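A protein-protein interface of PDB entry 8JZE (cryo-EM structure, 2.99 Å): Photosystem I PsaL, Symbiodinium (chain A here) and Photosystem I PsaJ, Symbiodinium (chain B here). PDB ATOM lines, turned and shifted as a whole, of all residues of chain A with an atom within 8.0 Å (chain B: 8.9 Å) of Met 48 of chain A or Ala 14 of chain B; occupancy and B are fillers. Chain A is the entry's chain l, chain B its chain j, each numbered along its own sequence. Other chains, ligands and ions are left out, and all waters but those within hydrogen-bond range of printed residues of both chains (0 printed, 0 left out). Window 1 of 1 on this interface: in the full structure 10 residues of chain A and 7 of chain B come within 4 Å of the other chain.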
ATOM      1  N   TYR A   4     -19.633 -40.902  11.517  1.00  0.00           N
ATOM      2  CA  TYR A   4     -19.542 -40.142  10.274  1.00  0.00           C
ATOM      3  C   TYR A   4     -19.682 -41.004   9.026  1.00  0.00           C
ATOM      4  O   TYR A   4     -19.803 -40.451   7.928  1.00  0.00           O
ATOM      5  CB  TYR A   4     -18.221 -39.366  10.217  1.00  0.00           C
ATOM      6  CG  TYR A   4     -16.982 -40.216  10.034  1.00  0.00           C
ATOM      7  CD1 TYR A   4     -16.511 -40.531   8.765  1.00  0.00           C
ATOM      8  CD2 TYR A   4     -16.271 -40.684  11.130  1.00  0.00           C
ATOM      9  CE1 TYR A   4     -15.379 -41.299   8.594  1.00  0.00           C
ATOM     10  CE2 TYR A   4     -15.134 -41.449  10.968  1.00  0.00           C
ATOM     11  CZ  TYR A   4     -14.696 -41.755   9.698  1.00  0.00           C
ATOM     12  OH  TYR A   4     -13.565 -42.520   9.531  1.00  0.00           O
ATOM     13  N   ILE A  12     -21.132 -36.376  -1.727  1.00  0.00           N
ATOM     14  CA  ILE A  12     -19.807 -36.270  -1.124  1.00  0.00           C
ATOM     15  C   ILE A  12     -18.909 -37.398  -1.615  1.00  0.00           C
ATOM     16  O   ILE A  12     -17.771 -37.167  -2.042  1.00  0.00           O
ATOM     17  CB  ILE A  12     -19.913 -36.253   0.411  1.00  0.00           C
ATOM     18  CG1 ILE A  12     -20.675 -35.009   0.872  1.00  0.00           C
ATOM     19  CG2 ILE A  12     -18.531 -36.303   1.044  1.00  0.00           C
ATOM     20  CD1 ILE A  12     -20.750 -34.858   2.373  1.00  0.00           C
ATOM     21  N   THR A  41     -10.173 -37.169   4.831  1.00  0.00           N
ATOM     22  CA  THR A  41     -10.958 -36.130   4.175  1.00  0.00           C
ATOM     23  C   THR A  41     -12.446 -36.457   4.222  1.00  0.00           C
ATOM     24  O   THR A  41     -13.280 -35.564   4.423  1.00  0.00           O
ATOM     25  CB  THR A  41     -10.487 -35.946   2.734  1.00  0.00           C
ATOM     26  OG1 THR A  41      -9.056 -35.866   2.706  1.00  0.00           O
ATOM     27  CG2 THR A  41     -11.061 -34.670   2.149  1.00  0.00           C
ATOM     28  N   VAL A  42     -12.794 -37.738   4.050  1.00  0.00           N
ATOM     29  CA  VAL A  42     -14.195 -38.146   4.142  1.00  0.00           C
ATOM     30  C   VAL A  42     -14.760 -37.813   5.516  1.00  0.00           C
ATOM     31  O   VAL A  42     -15.893 -37.338   5.636  1.00  0.00           O
ATOM     32  CB  VAL A  42     -14.342 -39.645   3.816  1.00  0.00           C
ATOM     33  CG1 VAL A  42     -15.710 -40.153   4.240  1.00  0.00           C
ATOM     34  CG2 VAL A  42     -14.138 -39.884   2.335  1.00  0.00           C
ATOM     35  N   LYS A  43     -13.985 -38.056   6.575  1.00  0.00           N
ATOM     36  CA  LYS A  43     -14.450 -37.712   7.915  1.00  0.00           C
ATOM     37  C   LYS A  43     -14.523 -36.203   8.105  1.00  0.00           C
ATOM     38  O   LYS A  43     -15.505 -35.686   8.649  1.00  0.00           O
ATOM     39  CB  LYS A  43     -13.542 -38.330   8.978  1.00  0.00           C
ATOM     40  CG  LYS A  43     -14.024 -38.080  10.402  1.00  0.00           C
ATOM     41  CD  LYS A  43     -13.017 -38.540  11.443  1.00  0.00           C
ATOM     42  CE  LYS A  43     -11.832 -37.594  11.522  1.00  0.00           C
ATOM     43  NZ  LYS A  43     -10.865 -38.004  12.576  1.00  0.00           N
ATOM     44  N   ALA A  44     -13.495 -35.479   7.660  1.00  0.00           N
ATOM     45  CA  ALA A  44     -13.445 -34.040   7.868  1.00  0.00           C
ATOM     46  C   ALA A  44     -14.516 -33.299   7.083  1.00  0.00           C
ATOM     47  O   ALA A  44     -14.799 -32.140   7.397  1.00  0.00           O
ATOM     48  CB  ALA A  44     -12.064 -33.501   7.493  1.00  0.00           C
ATOM     49  N   PHE A  45     -15.102 -33.925   6.066  1.00  0.00           N
ATOM     50  CA  PHE A  45     -16.182 -33.293   5.316  1.00  0.00           C
ATOM     51  C   PHE A  45     -17.564 -33.834   5.647  1.00  0.00           C
ATOM     52  O   PHE A  45     -18.512 -33.052   5.752  1.00  0.00           O
ATOM     53  CB  PHE A  45     -15.928 -33.427   3.811  1.00  0.00           C
ATOM     54  CG  PHE A  45     -15.035 -32.355   3.258  1.00  0.00           C
ATOM     55  CD1 PHE A  45     -13.660 -32.445   3.383  1.00  0.00           C
ATOM     56  CD2 PHE A  45     -15.575 -31.251   2.620  1.00  0.00           C
ATOM     57  CE1 PHE A  45     -12.838 -31.455   2.879  1.00  0.00           C
ATOM     58  CE2 PHE A  45     -14.762 -30.259   2.111  1.00  0.00           C
ATOM     59  CZ  PHE A  45     -13.390 -30.362   2.240  1.00  0.00           C
ATOM     60  N   ALA A  46     -17.712 -35.149   5.820  1.00  0.00           N
ATOM     61  CA  ALA A  46     -19.007 -35.722   6.171  1.00  0.00           C
ATOM     62  C   ALA A  46     -19.495 -35.252   7.532  1.00  0.00           C
ATOM     63  O   ALA A  46     -20.697 -35.322   7.806  1.00  0.00           O
ATOM     64  CB  ALA A  46     -18.934 -37.249   6.144  1.00  0.00           C
ATOM     65  N   GLU A  47     -18.590 -34.788   8.393  1.00  0.00           N
ATOM     66  CA  GLU A  47     -18.981 -34.186   9.658  1.00  0.00           C
ATOM     67  C   GLU A  47     -19.347 -32.715   9.516  1.00  0.00           C
ATOM     68  O   GLU A  47     -19.771 -32.102  10.501  1.00  0.00           O
ATOM     69  CB  GLU A  47     -17.860 -34.351  10.689  1.00  0.00           C
ATOM     70  CG  GLU A  47     -17.695 -35.781  11.191  1.00  0.00           C
ATOM     71  CD  GLU A  47     -16.549 -35.935  12.174  1.00  0.00           C
ATOM     72  OE1 GLU A  47     -15.472 -35.350  11.936  1.00  0.00           O
ATOM     73  OE2 GLU A  47     -16.728 -36.642  13.188  1.00  0.00           O
ATOM     74  N   MET A  48     -19.188 -32.140   8.326  1.00  0.00           N
ATOM     75  CA  MET A  48     -19.610 -30.775   8.036  1.00  0.00           C
ATOM     76  C   MET A  48     -20.798 -30.705   7.097  1.00  0.00           C
ATOM     77  O   MET A  48     -21.651 -29.828   7.252  1.00  0.00           O
ATOM     78  CB  MET A  48     -18.455 -29.974   7.425  1.00  0.00           C
ATOM     79  CG  MET A  48     -17.121 -30.220   8.084  1.00  0.00           C
ATOM     80  SD  MET A  48     -17.243 -30.163   9.874  1.00  0.00           S
ATOM     81  CE  MET A  48     -15.778 -31.080  10.343  1.00  0.00           C
ATOM     82  N   TYR A  49     -20.871 -31.601   6.118  1.00  0.00           N
ATOM     83  CA  TYR A  49     -21.932 -31.602   5.122  1.00  0.00           C
ATOM     84  C   TYR A  49     -22.718 -32.899   5.228  1.00  0.00           C
ATOM     85  O   TYR A  49     -22.131 -33.985   5.268  1.00  0.00           O
ATOM     86  CB  TYR A  49     -21.357 -31.428   3.715  1.00  0.00           C
ATOM     87  CG  TYR A  49     -20.489 -30.199   3.571  1.00  0.00           C
ATOM     88  CD1 TYR A  49     -21.048 -28.928   3.573  1.00  0.00           C
ATOM     89  CD2 TYR A  49     -19.111 -30.307   3.435  1.00  0.00           C
ATOM     90  CE1 TYR A  49     -20.262 -27.802   3.445  1.00  0.00           C
ATOM     91  CE2 TYR A  49     -18.316 -29.187   3.305  1.00  0.00           C
ATOM     92  CZ  TYR A  49     -18.898 -27.937   3.312  1.00  0.00           C
ATOM     93  OH  TYR A  49     -18.112 -26.816   3.182  1.00  0.00           O
ATOM     94  N   GLY A  50     -24.042 -32.782   5.275  1.00  0.00           N
ATOM     95  CA  GLY A  50     -24.906 -33.929   5.412  1.00  0.00           C
ATOM     96  C   GLY A  50     -26.356 -33.536   5.602  1.00  0.00           C
ATOM     97  O   GLY A  50     -26.744 -32.383   5.392  1.00  0.00           O
ATOM     98  N   PRO A  51     -27.190 -34.501   6.000  1.00  0.00           N
ATOM     99  CA  PRO A  51     -28.624 -34.196   6.169  1.00  0.00           C
ATOM    100  C   PRO A  51     -28.904 -33.167   7.253  1.00  0.00           C
ATOM    101  O   PRO A  51     -29.632 -32.197   7.009  1.00  0.00           O
ATOM    102  CB  PRO A  51     -29.229 -35.568   6.504  1.00  0.00           C
ATOM    103  CG  PRO A  51     -28.257 -36.560   5.952  1.00  0.00           C
ATOM    104  CD  PRO A  51     -26.908 -35.938   6.142  1.00  0.00           C
ATOM    105  N   GLY A  52     -28.349 -33.350   8.445  1.00  0.00           N
ATOM    106  CA  GLY A  52     -28.557 -32.429   9.542  1.00  0.00           C
ATOM    107  C   GLY A  52     -27.601 -31.258   9.582  1.00  0.00           C
ATOM    108  O   GLY A  52     -27.639 -30.471  10.534  1.00  0.00           O
ATOM    109  N   LYS A  53     -26.746 -31.116   8.573  1.00  0.00           N
ATOM    110  CA  LYS A  53     -25.701 -30.101   8.562  1.00  0.00           C
ATOM    111  C   LYS A  53     -25.789 -29.274   7.287  1.00  0.00           C
ATOM    112  O   LYS A  53     -26.801 -29.324   6.583  1.00  0.00           O
ATOM    113  CB  LYS A  53     -24.323 -30.752   8.689  1.00  0.00           C
ATOM    114  CG  LYS A  53     -24.239 -31.806   9.780  1.00  0.00           C
ATOM    115  CD  LYS A  53     -22.885 -32.486   9.792  1.00  0.00           C
ATOM    116  CE  LYS A  53     -22.907 -33.736  10.657  1.00  0.00           C
ATOM    117  NZ  LYS A  53     -23.880 -34.740  10.146  1.00  0.00           N
ATOM    118  N   ALA A  54     -24.749 -28.488   7.002  1.00  0.00           N
ATOM    119  CA  ALA A  54     -24.690 -27.695   5.780  1.00  0.00           C
ATOM    120  C   ALA A  54     -24.953 -28.559   4.554  1.00  0.00           C
ATOM    121  O   ALA A  54     -24.155 -29.441   4.224  1.00  0.00           O
ATOM    122  CB  ALA A  54     -23.329 -27.008   5.658  1.00  0.00           C
ATOM    123  N   THR A  55     -26.069 -28.309   3.875  1.00  0.00           N
ATOM    124  CA  THR A  55     -26.489 -29.112   2.734  1.00  0.00           C
ATOM    125  C   THR A  55     -26.042 -28.536   1.397  1.00  0.00           C
ATOM    126  O   THR A  55     -26.354 -29.121   0.355  1.00  0.00           O
ATOM    127  CB  THR A  55     -28.014 -29.265   2.731  1.00  0.00           C
ATOM    128  OG1 THR A  55     -28.626 -27.970   2.727  1.00  0.00           O
ATOM    129  CG2 THR A  55     -28.479 -30.034   3.956  1.00  0.00           C
ATOM    130  N   LYS A  56     -25.329 -27.414   1.394  1.00  0.00           N
ATOM    131  CA  LYS A  56     -24.900 -26.777   0.159  1.00  0.00           C
ATOM    132  C   LYS A  56     -23.440 -26.370   0.280  1.00  0.00           C
ATOM    133  O   LYS A  56     -22.915 -26.172   1.378  1.00  0.00           O
ATOM    134  CB  LYS A  56     -25.770 -25.558  -0.182  1.00  0.00           C
ATOM    135  CG  LYS A  56     -27.178 -25.910  -0.623  1.00  0.00           C
ATOM    136  CD  LYS A  56     -28.034 -24.670  -0.807  1.00  0.00           C
ATOM    137  CE  LYS A  56     -29.420 -25.039  -1.306  1.00  0.00           C
ATOM    138  NZ  LYS A  56     -30.032 -26.120  -0.484  1.00  0.00           N
ATOM    139  N   MET A  57     -22.784 -26.264  -0.872  1.00  0.00           N
ATOM    140  CA  MET A  57     -21.399 -25.829  -0.943  1.00  0.00           C
ATOM    141  C   MET A  57     -21.240 -24.876  -2.116  1.00  0.00           C
ATOM    142  O   MET A  57     -21.994 -24.926  -3.089  1.00  0.00           O
ATOM    143  CB  MET A  57     -20.435 -27.011  -1.111  1.00  0.00           C
ATOM    144  CG  MET A  57     -19.473 -27.200   0.041  1.00  0.00           C
ATOM    145  SD  MET A  57     -18.211 -28.438  -0.311  1.00  0.00           S
ATOM    146  CE  MET A  57     -19.225 -29.803  -0.865  1.00  0.00           C
ATOM    147  N   ILE B   9     -17.959 -19.540  11.425  1.00  0.00           N
ATOM    148  CA  ILE B   9     -18.476 -20.479  12.410  1.00  0.00           C
ATOM    149  C   ILE B   9     -17.611 -21.732  12.409  1.00  0.00           C
ATOM    150  O   ILE B   9     -16.902 -22.029  11.445  1.00  0.00           O
ATOM    151  CB  ILE B   9     -19.952 -20.848  12.152  1.00  0.00           C
ATOM    152  CG1 ILE B   9     -20.108 -21.510  10.785  1.00  0.00           C
ATOM    153  CG2 ILE B   9     -20.830 -19.617  12.248  1.00  0.00           C
ATOM    154  CD1 ILE B   9     -21.523 -21.943  10.476  1.00  0.00           C
ATOM    155  N   LYS B  10     -17.681 -22.466  13.512  1.00  0.00           N
ATOM    156  CA  LYS B  10     -16.922 -23.677  13.772  1.00  0.00           C
ATOM    157  C   LYS B  10     -17.657 -24.900  13.229  1.00  0.00           C
ATOM    158  O   LYS B  10     -18.885 -24.885  13.095  1.00  0.00           O
ATOM    159  CB  LYS B  10     -16.687 -23.839  15.273  1.00  0.00           C
ATOM    160  CG  LYS B  10     -15.356 -24.476  15.643  1.00  0.00           C
ATOM    161  CD  LYS B  10     -14.192 -23.726  15.012  1.00  0.00           C
ATOM    162  CE  LYS B  10     -12.886 -24.484  15.192  1.00  0.00           C
ATOM    163  NZ  LYS B  10     -11.753 -23.816  14.497  1.00  0.00           N
ATOM    164  N   PRO B  11     -16.911 -25.955  12.884  1.00  0.00           N
ATOM    165  CA  PRO B  11     -17.529 -27.215  12.447  1.00  0.00           C
ATOM    166  C   PRO B  11     -18.689 -27.707  13.300  1.00  0.00           C
ATOM    167  O   PRO B  11     -19.629 -28.313  12.775  1.00  0.00           O
ATOM    168  CB  PRO B  11     -16.357 -28.200  12.515  1.00  0.00           C
ATOM    169  CG  PRO B  11     -15.113 -27.350  12.352  1.00  0.00           C
ATOM    170  CD  PRO B  11     -15.496 -25.897  12.483  1.00  0.00           C
ATOM    171  N   GLU B  12     -18.632 -27.468  14.612  1.00  0.00           N
ATOM    172  CA  GLU B  12     -19.664 -27.976  15.511  1.00  0.00           C
ATOM    173  C   GLU B  12     -21.042 -27.401  15.209  1.00  0.00           C
ATOM    174  O   GLU B  12     -22.050 -28.018  15.569  1.00  0.00           O
ATOM    175  CB  GLU B  12     -19.287 -27.680  16.965  1.00  0.00           C
ATOM    176  CG  GLU B  12     -18.235 -28.615  17.555  1.00  0.00           C
ATOM    177  CD  GLU B  12     -16.846 -28.395  16.982  1.00  0.00           C
ATOM    178  OE1 GLU B  12     -16.632 -27.372  16.299  1.00  0.00           O
ATOM    179  OE2 GLU B  12     -15.964 -29.247  17.218  1.00  0.00           O
ATOM    180  N   GLU B  13     -21.112 -26.244  14.557  1.00  0.00           N
ATOM    181  CA  GLU B  13     -22.371 -25.589  14.226  1.00  0.00           C
ATOM    182  C   GLU B  13     -22.517 -25.416  12.719  1.00  0.00           C
ATOM    183  O   GLU B  13     -22.922 -24.360  12.231  1.00  0.00           O
ATOM    184  CB  GLU B  13     -22.491 -24.245  14.944  1.00  0.00           C
ATOM    185  CG  GLU B  13     -21.338 -23.273  14.701  1.00  0.00           C
ATOM    186  CD  GLU B  13     -20.166 -23.488  15.640  1.00  0.00           C
ATOM    187  OE1 GLU B  13     -19.797 -24.656  15.883  1.00  0.00           O
ATOM    188  OE2 GLU B  13     -19.616 -22.485  16.141  1.00  0.00           O
ATOM    189  N   ALA B  14     -22.185 -26.466  11.963  1.00  0.00           N
ATOM    190  CA  ALA B  14     -22.242 -26.382  10.506  1.00  0.00           C
ATOM    191  C   ALA B  14     -23.666 -26.131  10.023  1.00  0.00           C
ATOM    192  O   ALA B  14     -23.898 -25.286   9.150  1.00  0.00           O
ATOM    193  CB  ALA B  14     -21.682 -27.661   9.886  1.00  0.00           C
ATOM    194  N   GLY B  15     -24.631 -26.854  10.576  1.00  0.00           N
ATOM    195  CA  GLY B  15     -26.024 -26.696  10.222  1.00  0.00           C
ATOM    196  C   GLY B  15     -26.865 -25.939  11.226  1.00  0.00           C
ATOM    197  O   GLY B  15     -28.095 -25.935  11.099  1.00  0.00           O
ATOM    198  N   LYS B  16     -26.250 -25.299  12.218  1.00  0.00           N
ATOM    199  CA  LYS B  16     -26.979 -24.596  13.267  1.00  0.00           C
ATOM    200  C   LYS B  16     -27.032 -23.092  13.032  1.00  0.00           C
ATOM    201  O   LYS B  16     -28.105 -22.488  13.124  1.00  0.00           O
ATOM    202  CB  LYS B  16     -26.346 -24.890  14.634  1.00  0.00           C
ATOM    203  CG  LYS B  16     -25.969 -26.348  14.850  1.00  0.00           C
ATOM    204  CD  LYS B  16     -27.160 -27.274  14.666  1.00  0.00           C
ATOM    205  CE  LYS B  16     -26.746 -28.730  14.795  1.00  0.00           C
ATOM    206  NZ  LYS B  16     -25.655 -29.084  13.844  1.00  0.00           N
ATOM    207  N   ILE B  17     -25.896 -22.475  12.726  1.00  0.00           N
ATOM    208  CA  ILE B  17     -25.851 -21.041  12.465  1.00  0.00           C
ATOM    209  C   ILE B  17     -26.343 -20.779  11.047  1.00  0.00           C
ATOM    210  O   ILE B  17     -25.925 -21.451  10.097  1.00  0.00           O
ATOM    211  CB  ILE B  17     -24.429 -20.494  12.670  1.00  0.00           C
ATOM    212  CG1 ILE B  17     -23.913 -20.855  14.063  1.00  0.00           C
ATOM    213  CG2 ILE B  17     -24.408 -18.986  12.469  1.00  0.00           C
ATOM    214  CD1 ILE B  17     -24.737 -20.279  15.192  1.00  0.00           C
ATOM    215  N   THR B  18     -27.239 -19.803  10.904  1.00  0.00           N
ATOM    216  CA  THR B  18     -27.786 -19.436   9.604  1.00  0.00           C
ATOM    217  C   THR B  18     -27.749 -17.940   9.315  1.00  0.00           C
ATOM    218  O   THR B  18     -27.829 -17.563   8.140  1.00  0.00           O
ATOM    219  CB  THR B  18     -29.233 -19.936   9.470  1.00  0.00           C
ATOM    220  OG1 THR B  18     -29.332 -21.253  10.025  1.00  0.00           O
ATOM    221  CG2 THR B  18     -29.658 -19.997   8.008  1.00  0.00           C
ATOM    222  N   PRO B  26     -23.699 -16.827   2.996  1.00  0.00           N
ATOM    223  CA  PRO B  26     -23.955 -17.728   4.123  1.00  0.00           C
ATOM    224  C   PRO B  26     -22.715 -17.882   4.984  1.00  0.00           C
ATOM    225  O   PRO B  26     -21.601 -17.574   4.535  1.00  0.00           O
ATOM    226  CB  PRO B  26     -24.333 -19.051   3.436  1.00  0.00           C
ATOM    227  CG  PRO B  26     -23.698 -18.973   2.094  1.00  0.00           C
ATOM    228  CD  PRO B  26     -23.760 -17.527   1.702  1.00  0.00           C
ATOM    229  N   PRO B  27     -22.863 -18.338   6.230  1.00  0.00           N
ATOM    230  CA  PRO B  27     -21.691 -18.466   7.105  1.00  0.00           C
ATOM    231  C   PRO B  27     -20.668 -19.441   6.543  1.00  0.00           C
ATOM    232  O   PRO B  27     -21.007 -20.417   5.870  1.00  0.00           O
ATOM    233  CB  PRO B  27     -22.285 -18.975   8.424  1.00  0.00           C
ATOM    234  CG  PRO B  27     -23.581 -19.603   8.042  1.00  0.00           C
ATOM    235  CD  PRO B  27     -24.097 -18.775   6.905  1.00  0.00           C
ATOM    236  N   ARG B  28     -19.401 -19.159   6.824  1.00  0.00           N
ATOM    237  CA  ARG B  28     -18.290 -19.967   6.343  1.00  0.00           C
ATOM    238  C   ARG B  28     -17.706 -20.794   7.480  1.00  0.00           C
ATOM    239  O   ARG B  28     -17.505 -20.292   8.589  1.00  0.00           O
ATOM    240  CB  ARG B  28     -17.199 -19.087   5.728  1.00  0.00           C
ATOM    241  CG  ARG B  28     -17.669 -18.225   4.567  1.00  0.00           C
ATOM    242  CD  ARG B  28     -16.538 -17.375   4.012  1.00  0.00           C
ATOM    243  NE  ARG B  28     -15.417 -18.187   3.554  1.00  0.00           N
ATOM    244  CZ  ARG B  28     -15.314 -18.704   2.337  1.00  0.00           C
ATOM    245  NH1 ARG B  28     -16.249 -18.513   1.423  1.00  0.00           N
ATOM    246  NH2 ARG B  28     -14.244 -19.433   2.031  1.00  0.00           N
ATOM    247  N   ILE B  29     -17.436 -22.063   7.196  1.00  0.00           N
ATOM    248  CA  ILE B  29     -16.828 -22.969   8.164  1.00  0.00           C
ATOM    249  C   ILE B  29     -15.324 -22.736   8.168  1.00  0.00           C
ATOM    250  O   ILE B  29     -14.685 -22.740   7.110  1.00  0.00           O
ATOM    251  CB  ILE B  29     -17.153 -24.433   7.828  1.00  0.00           C
ATOM    252  CG1 ILE B  29     -18.650 -24.617   7.572  1.00  0.00           C
ATOM    253  CG2 ILE B  29     -16.680 -25.352   8.945  1.00  0.00           C
ATOM    254  CD1 ILE B  29     -19.501 -24.490   8.809  1.00  0.00           C
ATOM    255  N   VAL B  30     -14.755 -22.535   9.352  1.00  0.00           N
ATOM    256  CA  VAL B  30     -13.313 -22.383   9.509  1.00  0.00           C
ATOM    257  C   VAL B  30     -12.750 -23.701  10.021  1.00  0.00           C
ATOM    258  O   VAL B  30     -13.171 -24.204  11.069  1.00  0.00           O
ATOM    259  CB  VAL B  30     -12.960 -21.219  10.451  1.00  0.00           C
ATOM    260  CG1 VAL B  30     -13.758 -21.299  11.741  1.00  0.00           C
ATOM    261  CG2 VAL B  30     -11.468 -21.209  10.746  1.00  0.00           C
ATOM    262  N   VAL B  31     -11.810 -24.273   9.275  1.00  0.00           N
ATOM    263  CA  VAL B  31     -11.146 -25.515   9.653  1.00  0.00           C
ATOM    264  C   VAL B  31      -9.719 -25.168  10.047  1.00  0.00           C
ATOM    265  O   VAL B  31      -8.969 -24.595   9.247  1.00  0.00           O
ATOM    266  CB  VAL B  31     -11.174 -26.548   8.517  1.00  0.00           C
ATOM    267  CG1 VAL B  31     -10.544 -27.853   8.974  1.00  0.00           C
ATOM    268  CG2 VAL B  31     -12.596 -26.784   8.046  1.00  0.00           C
ATOM    269  N   LYS B  32      -9.345 -25.510  11.277  1.00  0.00           N
ATOM    270  CA  LYS B  32      -8.022 -25.184  11.807  1.00  0.00           C
ATOM    271  C   LYS B  32      -7.057 -26.286  11.393  1.00  0.00           C
ATOM    272  O   LYS B  32      -6.840 -27.260  12.115  1.00  0.00           O
ATOM    273  CB  LYS B  32      -8.075 -25.011  13.320  1.00  0.00           C
ATOM    274  CG  LYS B  32      -6.730 -24.724  13.973  1.00  0.00           C
ATOM    275  CD  LYS B  32      -6.096 -23.458  13.421  1.00  0.00           C
ATOM    276  CE  LYS B  32      -4.724 -23.219  14.032  1.00  0.00           C
ATOM    277  NZ  LYS B  32      -3.790 -24.347  13.762  1.00  0.00           N
ATOM    278  N   LEU B  43     -14.299 -22.940   4.568  1.00  0.00           N
ATOM    279  CA  LEU B  43     -15.208 -23.646   3.677  1.00  0.00           C
ATOM    280  C   LEU B  43     -16.542 -22.914   3.620  1.00  0.00           C
ATOM    281  O   LEU B  43     -17.008 -22.378   4.630  1.00  0.00           O
ATOM    282  CB  LEU B  43     -15.416 -25.090   4.142  1.00  0.00           C
ATOM    283  CG  LEU B  43     -14.137 -25.915   4.309  1.00  0.00           C
ATOM    284  CD1 LEU B  43     -14.447 -27.326   4.784  1.00  0.00           C
ATOM    285  CD2 LEU B  43     -13.354 -25.945   3.009  1.00  0.00           C
ATOM    286  N   SER B  44     -17.148 -22.885   2.440  1.00  0.00           N
ATOM    287  CA  SER B  44     -18.399 -22.169   2.246  1.00  0.00           C
ATOM    288  C   SER B  44     -19.595 -23.082   2.493  1.00  0.00           C
ATOM    289  O   SER B  44     -19.485 -24.310   2.509  1.00  0.00           O
ATOM    290  CB  SER B  44     -18.477 -21.581   0.836  1.00  0.00           C
ATOM    291  OG  SER B  44     -18.396 -22.599  -0.147  1.00  0.00           O
ATOM    292  N   THR B  45     -20.754 -22.453   2.693  1.00  0.00           N
ATOM    293  CA  THR B  45     -22.018 -23.148   2.877  1.00  0.00           C
ATOM    294  C   THR B  45     -22.970 -22.946   1.706  1.00  0.00           C
ATOM    295  O   THR B  45     -23.998 -23.628   1.632  1.00  0.00           O
ATOM    296  CB  THR B  45     -22.684 -22.680   4.183  1.00  0.00           C
ATOM    297  OG1 THR B  45     -21.701 -22.634   5.224  1.00  0.00           O
ATOM    298  CG2 THR B  45     -23.795 -23.625   4.613  1.00  0.00           C
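The backbone carbonyl oxygen of Ser 44 of chain B sits at hydrogen-bond distance from the side-chain hydroxyl of Tyr 49 of chain A (2.9 Å). The backbone carbonyl oxygen of Lys 56 of chain A lies close to the backbone carbonyl oxygen of Thr 45 of chain B, at 2.8 Å.
The backbone carbonyl oxygen (O) of Pro 27 of chain B is in hydrogen-bond range of the side-chain hydroxyl (OG1) of Thr 45 of chain B (2.4 Å). The backbone carbonyl oxygen (O) of Ile 29 of chain B lies within hydrogen-bond range of the backbone NH (N) of Leu 43 of chain B (2.6 Å). The backbone carbonyl oxygen (O) of Met 48 of chain A sits at hydrogen-bond distance from the backbone NH (N) of Ala 54 of chain A (3.4 Å).
CD1 of Leu 43 of chain B touches CE2 of Phe 45 of chain A (3.98 Å). Pro 11 of chain B touches Met 48 of chain A (CB to SD, 3.4 Å). Met 48 of chain A touches Ala 14 of chain B. OH of Tyr 49 of chain A touches CB of Leu 43 of chain B, at 3.3 Å. CA of Lys 53 of chain A touches CA of Gly 15 of chain B, 3.8 Å away. O of Ala 14 of chain B touches CB of Ala 54 of chain A (3.9 Å). CA of Gly 15 of chain B touches N of Ala 54 of chain A, 3.9 Å away. Ala 54 of chain A touches Thr 45 of chain B. Met 57 of chain A touches Ser 44 of chain B (CG to O, 3.8 Å). Met 57 of chain A touches Thr 45 of chain B.
Of chain B, only Pro 11 and Ala 14 come within 4 Å of Met 48 of chain A. Ala 54 of chain A touches three residues of chain B. Of the printed residues of chain B, Lys 56 of chain A touches Thr 45 (2.8 Å). Printed residues of chain B within 4 Å of Met 57 of chain A: Ser 44 and Thr 45. Ala 14 of chain B touches just these residues of chain A: Met 48 and Ala 54. Of the printed residues of chain A, Ser 44 of chain B touches Tyr 49 (2.9 Å) and Met 57 (3.8 Å). The nearest residue of chain A that does not touch Ala 14 of chain B is Lys 53 of chain A (4.2 Å). The nearest printed residue of chain A that does not touch Pro 11 of chain B is Glu 47 of chain A (4.4 Å).
Printed residues of chain A that touch a printed residue of chain B: Phe 45, Met 48, Tyr 49, Lys 53, Ala 54, Lys 56 and Met 57. Hydrophobic or aromatic side chains of chain A within 4 Å of the printed part of chain B: Phe 45, Met 48, Tyr 49, Ala 54 and Met 57. Hydrophobic or aromatic side chains of chain B that line the printed part of chain A: Pro 11, Ala 14 and Leu 43.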
